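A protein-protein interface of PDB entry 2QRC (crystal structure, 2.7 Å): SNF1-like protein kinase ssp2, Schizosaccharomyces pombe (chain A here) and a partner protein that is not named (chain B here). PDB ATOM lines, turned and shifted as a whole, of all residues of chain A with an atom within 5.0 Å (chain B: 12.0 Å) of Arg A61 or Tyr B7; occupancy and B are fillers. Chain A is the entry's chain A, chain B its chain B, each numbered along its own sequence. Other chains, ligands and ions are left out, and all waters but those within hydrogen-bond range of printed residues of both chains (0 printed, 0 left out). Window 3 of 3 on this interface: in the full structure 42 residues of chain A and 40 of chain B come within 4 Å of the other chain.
The backbone carbonyl oxygen (O) of Gln A40 lies within hydrogen-bond range of the backbone NH (N) of Arg A61, at 2.8 Å.
The backbone NH (N) of Thr A42 sits at hydrogen-bond distance from the backbone carbonyl oxygen (O) of Lys A59 (3.0 Å).
OG of Ser A60 lies within hydrogen-bond range of NE1 of Trp A62.
OG of Ser B8 is in hydrogen-bond range of N of Glu B10.
Hydrophobic or aromatic side chains of chain B that line the printed part of chain A: Tyr B7.
Of the 13 printed residues of chain A, 7 touch a printed residue of chain B.
Printed residues of chain A that touch a printed residue of chain B: Gln A40, Phe A41, Thr A42, Lys A59, Ser A60, Arg A61 and Tyr A77.
Among the printed residues, no Asp or Glu carboxylate lies within 4 Å of a Lys or Arg side-chain nitrogen of the other chain.
No residue of chain B comes within 4 Å of Gly A38.
Ala A39 touches none of the printed residues of chain B.
Of chain B, only Ser B8 comes within 4 Å of Gln A40.
Phe A41 touches just these residues of chain B: Tyr B7, Ser B8, Thr B9 and Glu B10.
Of chain B, only Gln B6 (3.8 Å) comes within 4 Å of Thr A42.
Ser A60 touches just one residue of chain B: Tyr B7.
Arg A61 touches just one residue of chain B: Tyr B7.
No residue of chain B comes within 4 Å of Trp A62.
No residue of chain B comes within 4 Å of Tyr A75.
No residue of chain B comes within 4 Å of Ala A76.
Of the printed residues of chain A, Gln B6 touches Thr A42 (3.8 Å).
Tyr B7 touches five residues of chain A.
Of the printed residues of chain A, Ser B8 touches Gln A40 and Phe A41.
Printed residues of chain A within 4 Å of Thr B9: Phe A41.
Printed residues of chain A within 4 Å of Glu B10: Phe A41 (3.5 Å).
Pro B12 touches none of the printed residues of chain A.
The nearest residue of chain B that does not touch Arg A61 is Ser B8 (6.9 Å).
The nearest residue of chain A that does not touch Tyr B7 is Gln A40 (4.1 Å).
The nearest printed residue of chain A that does not touch Ser B8 is Thr A42 (4.7 Å).
The backbone carbonyl oxygen (O) of Phe A41 is in hydrogen-bond range of the backbone NH (N) of Ser B8 (2.8 Å).
O of Ser B8 touches CA of Gln A40, 3.4 Å away.
Phe A41 touches Tyr B7.
Thr B9 touches Phe A41.
Phe A41 touches Glu B10.
CG2 of Thr A42 touches O of Gln B6, at 3.8 Å.
O of Lys A59 touches CE2 of Tyr B7 (3.6 Å).
Tyr B7 touches Ser A60.
Arg A61 touches Tyr B7 (NH1 to CD1, 3.4 Å).
CD1 of Tyr A77 touches OH of Tyr B7 (3.2 Å).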
ATOM      1  N   GLY A  38     -11.942  -9.683  23.945  1.00  0.00           N
ATOM      2  CA  GLY A  38     -12.436 -10.980  24.405  1.00  0.00           C
ATOM      3  C   GLY A  38     -13.561 -10.829  25.417  1.00  0.00           C
ATOM      4  O   GLY A  38     -13.829 -11.721  26.214  1.00  0.00           O
ATOM      5  N   ALA A  39     -14.220  -9.680  25.402  1.00  0.00           N
ATOM      6  CA  ALA A  39     -15.416  -9.512  26.185  1.00  0.00           C
ATOM      7  C   ALA A  39     -16.539 -10.221  25.430  1.00  0.00           C
ATOM      8  O   ALA A  39     -16.399 -10.552  24.238  1.00  0.00           O
ATOM      9  CB  ALA A  39     -15.712  -8.036  26.372  1.00  0.00           C
ATOM     10  N   GLN A  40     -17.636 -10.492  26.131  1.00  0.00           N
ATOM     11  CA  GLN A  40     -18.800 -11.075  25.495  1.00  0.00           C
ATOM     12  C   GLN A  40     -19.913 -10.106  25.728  1.00  0.00           C
ATOM     13  O   GLN A  40     -19.799  -9.281  26.604  1.00  0.00           O
ATOM     14  CB  GLN A  40     -19.087 -12.452  26.056  1.00  0.00           C
ATOM     15  CG  GLN A  40     -17.916 -13.410  25.814  1.00  0.00           C
ATOM     16  CD  GLN A  40     -18.304 -14.843  26.017  1.00  0.00           C
ATOM     17  OE1 GLN A  40     -19.464 -15.137  26.285  1.00  0.00           O
ATOM     18  NE2 GLN A  40     -17.337 -15.756  25.890  1.00  0.00           N
ATOM     19  N   PHE A  41     -20.967 -10.174  24.927  1.00  0.00           N
ATOM     20  CA  PHE A  41     -21.905  -9.069  24.816  1.00  0.00           C
ATOM     21  C   PHE A  41     -23.298  -9.492  24.377  1.00  0.00           C
ATOM     22  O   PHE A  41     -23.461 -10.482  23.656  1.00  0.00           O
ATOM     23  CB  PHE A  41     -21.368  -8.025  23.835  1.00  0.00           C
ATOM     24  CG  PHE A  41     -20.641  -8.613  22.643  1.00  0.00           C
ATOM     25  CD1 PHE A  41     -21.334  -9.054  21.529  1.00  0.00           C
ATOM     26  CD2 PHE A  41     -19.257  -8.713  22.637  1.00  0.00           C
ATOM     27  CE1 PHE A  41     -20.668  -9.593  20.432  1.00  0.00           C
ATOM     28  CE2 PHE A  41     -18.593  -9.254  21.534  1.00  0.00           C
ATOM     29  CZ  PHE A  41     -19.307  -9.697  20.434  1.00  0.00           C
ATOM     30  N   THR A  42     -24.296  -8.720  24.809  1.00  0.00           N
ATOM     31  CA  THR A  42     -25.626  -8.841  24.252  1.00  0.00           C
ATOM     32  C   THR A  42     -25.647  -8.196  22.881  1.00  0.00           C
ATOM     33  O   THR A  42     -24.740  -7.463  22.485  1.00  0.00           O
ATOM     34  CB  THR A  42     -26.695  -8.144  25.085  1.00  0.00           C
ATOM     35  OG1 THR A  42     -26.465  -6.745  25.032  1.00  0.00           O
ATOM     36  CG2 THR A  42     -26.678  -8.610  26.518  1.00  0.00           C
ATOM     37  N   LYS A  59     -24.779  -4.719  27.170  1.00  0.00           N
ATOM     38  CA  LYS A  59     -24.269  -5.329  28.389  1.00  0.00           C
ATOM     39  C   LYS A  59     -23.120  -6.255  28.025  1.00  0.00           C
ATOM     40  O   LYS A  59     -23.285  -7.152  27.214  1.00  0.00           O
ATOM     41  CB  LYS A  59     -25.377  -6.113  29.087  1.00  0.00           C
ATOM     42  CG  LYS A  59     -26.526  -5.254  29.573  1.00  0.00           C
ATOM     43  CD  LYS A  59     -27.051  -5.821  30.864  1.00  0.00           C
ATOM     44  CE  LYS A  59     -28.274  -5.097  31.346  1.00  0.00           C
ATOM     45  NZ  LYS A  59     -28.788  -5.885  32.485  1.00  0.00           N
ATOM     46  N   SER A  60     -21.952  -6.050  28.590  1.00  0.00           N
ATOM     47  CA  SER A  60     -20.851  -6.944  28.271  1.00  0.00           C
ATOM     48  C   SER A  60     -20.409  -7.704  29.517  1.00  0.00           C
ATOM     49  O   SER A  60     -20.750  -7.328  30.635  1.00  0.00           O
ATOM     50  CB  SER A  60     -19.666  -6.191  27.627  1.00  0.00           C
ATOM     51  OG  SER A  60     -19.041  -5.285  28.536  1.00  0.00           O
ATOM     52  N   ARG A  61     -19.653  -8.771  29.320  1.00  0.00           N
ATOM     53  CA  ARG A  61     -19.069  -9.521  30.408  1.00  0.00           C
ATOM     54  C   ARG A  61     -17.613  -9.825  30.090  1.00  0.00           C
ATOM     55  O   ARG A  61     -17.273 -10.328  28.999  1.00  0.00           O
ATOM     56  CB  ARG A  61     -19.832 -10.809  30.600  1.00  0.00           C
ATOM     57  CG  ARG A  61     -19.506 -11.543  31.869  1.00  0.00           C
ATOM     58  CD  ARG A  61     -20.301 -12.796  31.952  1.00  0.00           C
ATOM     59  NE  ARG A  61     -19.801 -13.825  31.056  1.00  0.00           N
ATOM     60  CZ  ARG A  61     -20.515 -14.888  30.694  1.00  0.00           C
ATOM     61  NH1 ARG A  61     -21.757 -15.042  31.155  1.00  0.00           N
ATOM     62  NH2 ARG A  61     -19.998 -15.798  29.878  1.00  0.00           N
ATOM     63  N   TRP A  62     -16.762  -9.531  31.058  1.00  0.00           N
ATOM     64  CA  TRP A  62     -15.332  -9.592  30.876  1.00  0.00           C
ATOM     65  C   TRP A  62     -14.731 -10.559  31.890  1.00  0.00           C
ATOM     66  O   TRP A  62     -15.027 -10.481  33.091  1.00  0.00           O
ATOM     67  CB  TRP A  62     -14.758  -8.216  31.109  1.00  0.00           C
ATOM     68  CG  TRP A  62     -15.215  -7.113  30.141  1.00  0.00           C
ATOM     69  CD1 TRP A  62     -16.474  -6.551  30.024  1.00  0.00           C
ATOM     70  CD2 TRP A  62     -14.384  -6.409  29.225  1.00  0.00           C
ATOM     71  NE1 TRP A  62     -16.466  -5.557  29.072  1.00  0.00           N
ATOM     72  CE2 TRP A  62     -15.201  -5.455  28.559  1.00  0.00           C
ATOM     73  CE3 TRP A  62     -13.027  -6.500  28.888  1.00  0.00           C
ATOM     74  CZ2 TRP A  62     -14.698  -4.594  27.573  1.00  0.00           C
ATOM     75  CZ3 TRP A  62     -12.523  -5.646  27.918  1.00  0.00           C
ATOM     76  CH2 TRP A  62     -13.361  -4.699  27.265  1.00  0.00           C
ATOM     77  N   GLU A  63     -13.921 -11.492  31.403  1.00  0.00           N
ATOM     78  CA  GLU A  63     -13.225 -12.421  32.270  1.00  0.00           C
ATOM     79  C   GLU A  63     -12.092 -11.615  32.878  1.00  0.00           C
ATOM     80  O   GLU A  63     -11.383 -10.937  32.160  1.00  0.00           O
ATOM     81  CB  GLU A  63     -12.707 -13.613  31.458  1.00  0.00           C
ATOM     82  CG  GLU A  63     -12.452 -14.870  32.301  1.00  0.00           C
ATOM     83  CD  GLU A  63     -12.796 -16.201  31.588  1.00  0.00           C
ATOM     84  OE1 GLU A  63     -12.531 -16.325  30.363  1.00  0.00           O
ATOM     85  OE2 GLU A  63     -13.315 -17.133  32.268  1.00  0.00           O
ATOM     86  N   TYR A  75     -15.961 -12.627  36.947  1.00  0.00           N
ATOM     87  CA  TYR A  75     -16.361 -11.887  35.757  1.00  0.00           C
ATOM     88  C   TYR A  75     -16.581 -10.446  36.137  1.00  0.00           C
ATOM     89  O   TYR A  75     -16.808 -10.154  37.307  1.00  0.00           O
ATOM     90  CB  TYR A  75     -17.644 -12.488  35.159  1.00  0.00           C
ATOM     91  CG  TYR A  75     -17.435 -13.864  34.546  1.00  0.00           C
ATOM     92  CD1 TYR A  75     -17.498 -15.012  35.323  1.00  0.00           C
ATOM     93  CD2 TYR A  75     -17.157 -14.007  33.187  1.00  0.00           C
ATOM     94  CE1 TYR A  75     -17.305 -16.259  34.770  1.00  0.00           C
ATOM     95  CE2 TYR A  75     -16.958 -15.253  32.623  1.00  0.00           C
ATOM     96  CZ  TYR A  75     -17.034 -16.373  33.421  1.00  0.00           C
ATOM     97  OH  TYR A  75     -16.847 -17.617  32.866  1.00  0.00           O
ATOM     98  N   ALA A  76     -16.490  -9.552  35.160  1.00  0.00           N
ATOM     99  CA  ALA A  76     -16.827  -8.158  35.378  1.00  0.00           C
ATOM    100  C   ALA A  76     -17.924  -7.720  34.394  1.00  0.00           C
ATOM    101  O   ALA A  76     -17.855  -7.984  33.196  1.00  0.00           O
ATOM    102  CB  ALA A  76     -15.606  -7.310  35.249  1.00  0.00           C
ATOM    103  N   TYR A  77     -18.944  -7.062  34.916  1.00  0.00           N
ATOM    104  CA  TYR A  77     -20.092  -6.675  34.137  1.00  0.00           C
ATOM    105  C   TYR A  77     -20.051  -5.183  33.806  1.00  0.00           C
ATOM    106  O   TYR A  77     -20.049  -4.314  34.689  1.00  0.00           O
ATOM    107  CB  TYR A  77     -21.344  -7.064  34.915  1.00  0.00           C
ATOM    108  CG  TYR A  77     -21.431  -8.571  35.102  1.00  0.00           C
ATOM    109  CD1 TYR A  77     -21.972  -9.374  34.108  1.00  0.00           C
ATOM    110  CD2 TYR A  77     -20.938  -9.197  36.256  1.00  0.00           C
ATOM    111  CE1 TYR A  77     -22.026 -10.733  34.252  1.00  0.00           C
ATOM    112  CE2 TYR A  77     -21.005 -10.578  36.406  1.00  0.00           C
ATOM    113  CZ  TYR A  77     -21.546 -11.326  35.398  1.00  0.00           C
ATOM    114  OH  TYR A  77     -21.613 -12.688  35.496  1.00  0.00           O
ATOM    115  N   GLN B   6     -28.607 -12.733  28.160  1.00  0.00           N
ATOM    116  CA  GLN B   6     -28.102 -13.695  27.189  1.00  0.00           C
ATOM    117  C   GLN B   6     -26.887 -13.147  26.449  1.00  0.00           C
ATOM    118  O   GLN B   6     -27.020 -12.318  25.548  1.00  0.00           O
ATOM    119  CB  GLN B   6     -29.198 -14.077  26.192  1.00  0.00           C
ATOM    120  CG  GLN B   6     -30.481 -14.574  26.839  1.00  0.00           C
ATOM    121  CD  GLN B   6     -30.547 -16.087  26.916  1.00  0.00           C
ATOM    122  OE1 GLN B   6     -29.523 -16.758  27.038  1.00  0.00           O
ATOM    123  NE2 GLN B   6     -31.757 -16.630  26.843  1.00  0.00           N
ATOM    124  N   TYR B   7     -25.705 -13.614  26.835  1.00  0.00           N
ATOM    125  CA  TYR B   7     -24.448 -13.131  26.235  1.00  0.00           C
ATOM    126  C   TYR B   7     -24.108 -13.757  24.873  1.00  0.00           C
ATOM    127  O   TYR B   7     -24.793 -14.668  24.431  1.00  0.00           O
ATOM    128  CB  TYR B   7     -23.289 -13.296  27.228  1.00  0.00           C
ATOM    129  CG  TYR B   7     -23.403 -12.335  28.384  1.00  0.00           C
ATOM    130  CD1 TYR B   7     -23.756 -12.774  29.654  1.00  0.00           C
ATOM    131  CD2 TYR B   7     -23.222 -10.976  28.185  1.00  0.00           C
ATOM    132  CE1 TYR B   7     -23.904 -11.896  30.690  1.00  0.00           C
ATOM    133  CE2 TYR B   7     -23.364 -10.091  29.206  1.00  0.00           C
ATOM    134  CZ  TYR B   7     -23.701 -10.554  30.459  1.00  0.00           C
ATOM    135  OH  TYR B   7     -23.814  -9.632  31.473  1.00  0.00           O
ATOM    136  N   SER B   8     -23.067 -13.245  24.205  1.00  0.00           N
ATOM    137  CA  SER B   8     -22.645 -13.734  22.881  1.00  0.00           C
ATOM    138  C   SER B   8     -21.228 -13.314  22.509  1.00  0.00           C
ATOM    139  O   SER B   8     -20.732 -12.280  22.932  1.00  0.00           O
ATOM    140  CB  SER B   8     -23.615 -13.272  21.782  1.00  0.00           C
ATOM    141  OG  SER B   8     -23.003 -13.299  20.500  1.00  0.00           O
ATOM    142  N   THR B   9     -20.603 -14.124  21.668  1.00  0.00           N
ATOM    143  CA  THR B   9     -19.218 -13.923  21.264  1.00  0.00           C
ATOM    144  C   THR B   9     -19.052 -13.317  19.858  1.00  0.00           C
ATOM    145  O   THR B   9     -17.971 -12.815  19.531  1.00  0.00           O
ATOM    146  CB  THR B   9     -18.441 -15.250  21.341  1.00  0.00           C
ATOM    147  OG1 THR B   9     -17.150 -15.080  20.756  1.00  0.00           O
ATOM    148  CG2 THR B   9     -19.182 -16.360  20.595  1.00  0.00           C
ATOM    149  N   GLU B  10     -20.108 -13.353  19.038  1.00  0.00           N
ATOM    150  CA  GLU B  10     -19.995 -12.936  17.634  1.00  0.00           C
ATOM    151  C   GLU B  10     -20.704 -11.635  17.205  1.00  0.00           C
ATOM    152  O   GLU B  10     -21.817 -11.345  17.650  1.00  0.00           O
ATOM    153  CB  GLU B  10     -20.373 -14.091  16.706  1.00  0.00           C
ATOM    154  CG  GLU B  10     -19.331 -15.236  16.658  1.00  0.00           C
ATOM    155  CD  GLU B  10     -17.919 -14.797  16.216  1.00  0.00           C
ATOM    156  OE1 GLU B  10     -17.728 -13.637  15.762  1.00  0.00           O
ATOM    157  OE2 GLU B  10     -16.997 -15.636  16.320  1.00  0.00           O
ATOM    158  N   ILE B  11     -20.018 -10.873  16.341  1.00  0.00           N
ATOM    159  CA  ILE B  11     -20.481  -9.603  15.734  1.00  0.00           C
ATOM    160  C   ILE B  11     -21.827  -9.711  15.007  1.00  0.00           C
ATOM    161  O   ILE B  11     -21.955 -10.500  14.073  1.00  0.00           O
ATOM    162  CB  ILE B  11     -19.419  -9.053  14.710  1.00  0.00           C
ATOM    163  CG1 ILE B  11     -18.650 -10.199  14.009  1.00  0.00           C
ATOM    164  CG2 ILE B  11     -18.422  -8.133  15.392  1.00  0.00           C
ATOM    165  CD1 ILE B  11     -19.296 -10.783  12.718  1.00  0.00           C
ATOM    166  N   PRO B  12     -22.837  -8.919  15.414  1.00  0.00           N
ATOM    167  CA  PRO B  12     -24.137  -9.099  14.748  1.00  0.00           C
ATOM    168  C   PRO B  12     -23.981  -8.922  13.248  1.00  0.00           C
ATOM    169  O   PRO B  12     -23.306  -7.982  12.801  1.00  0.00           O
ATOM    170  CB  PRO B  12     -25.012  -7.992  15.335  1.00  0.00           C
ATOM    171  CG  PRO B  12     -24.384  -7.663  16.634  1.00  0.00           C
ATOM    172  CD  PRO B  12     -22.891  -7.866  16.446  1.00  0.00           C
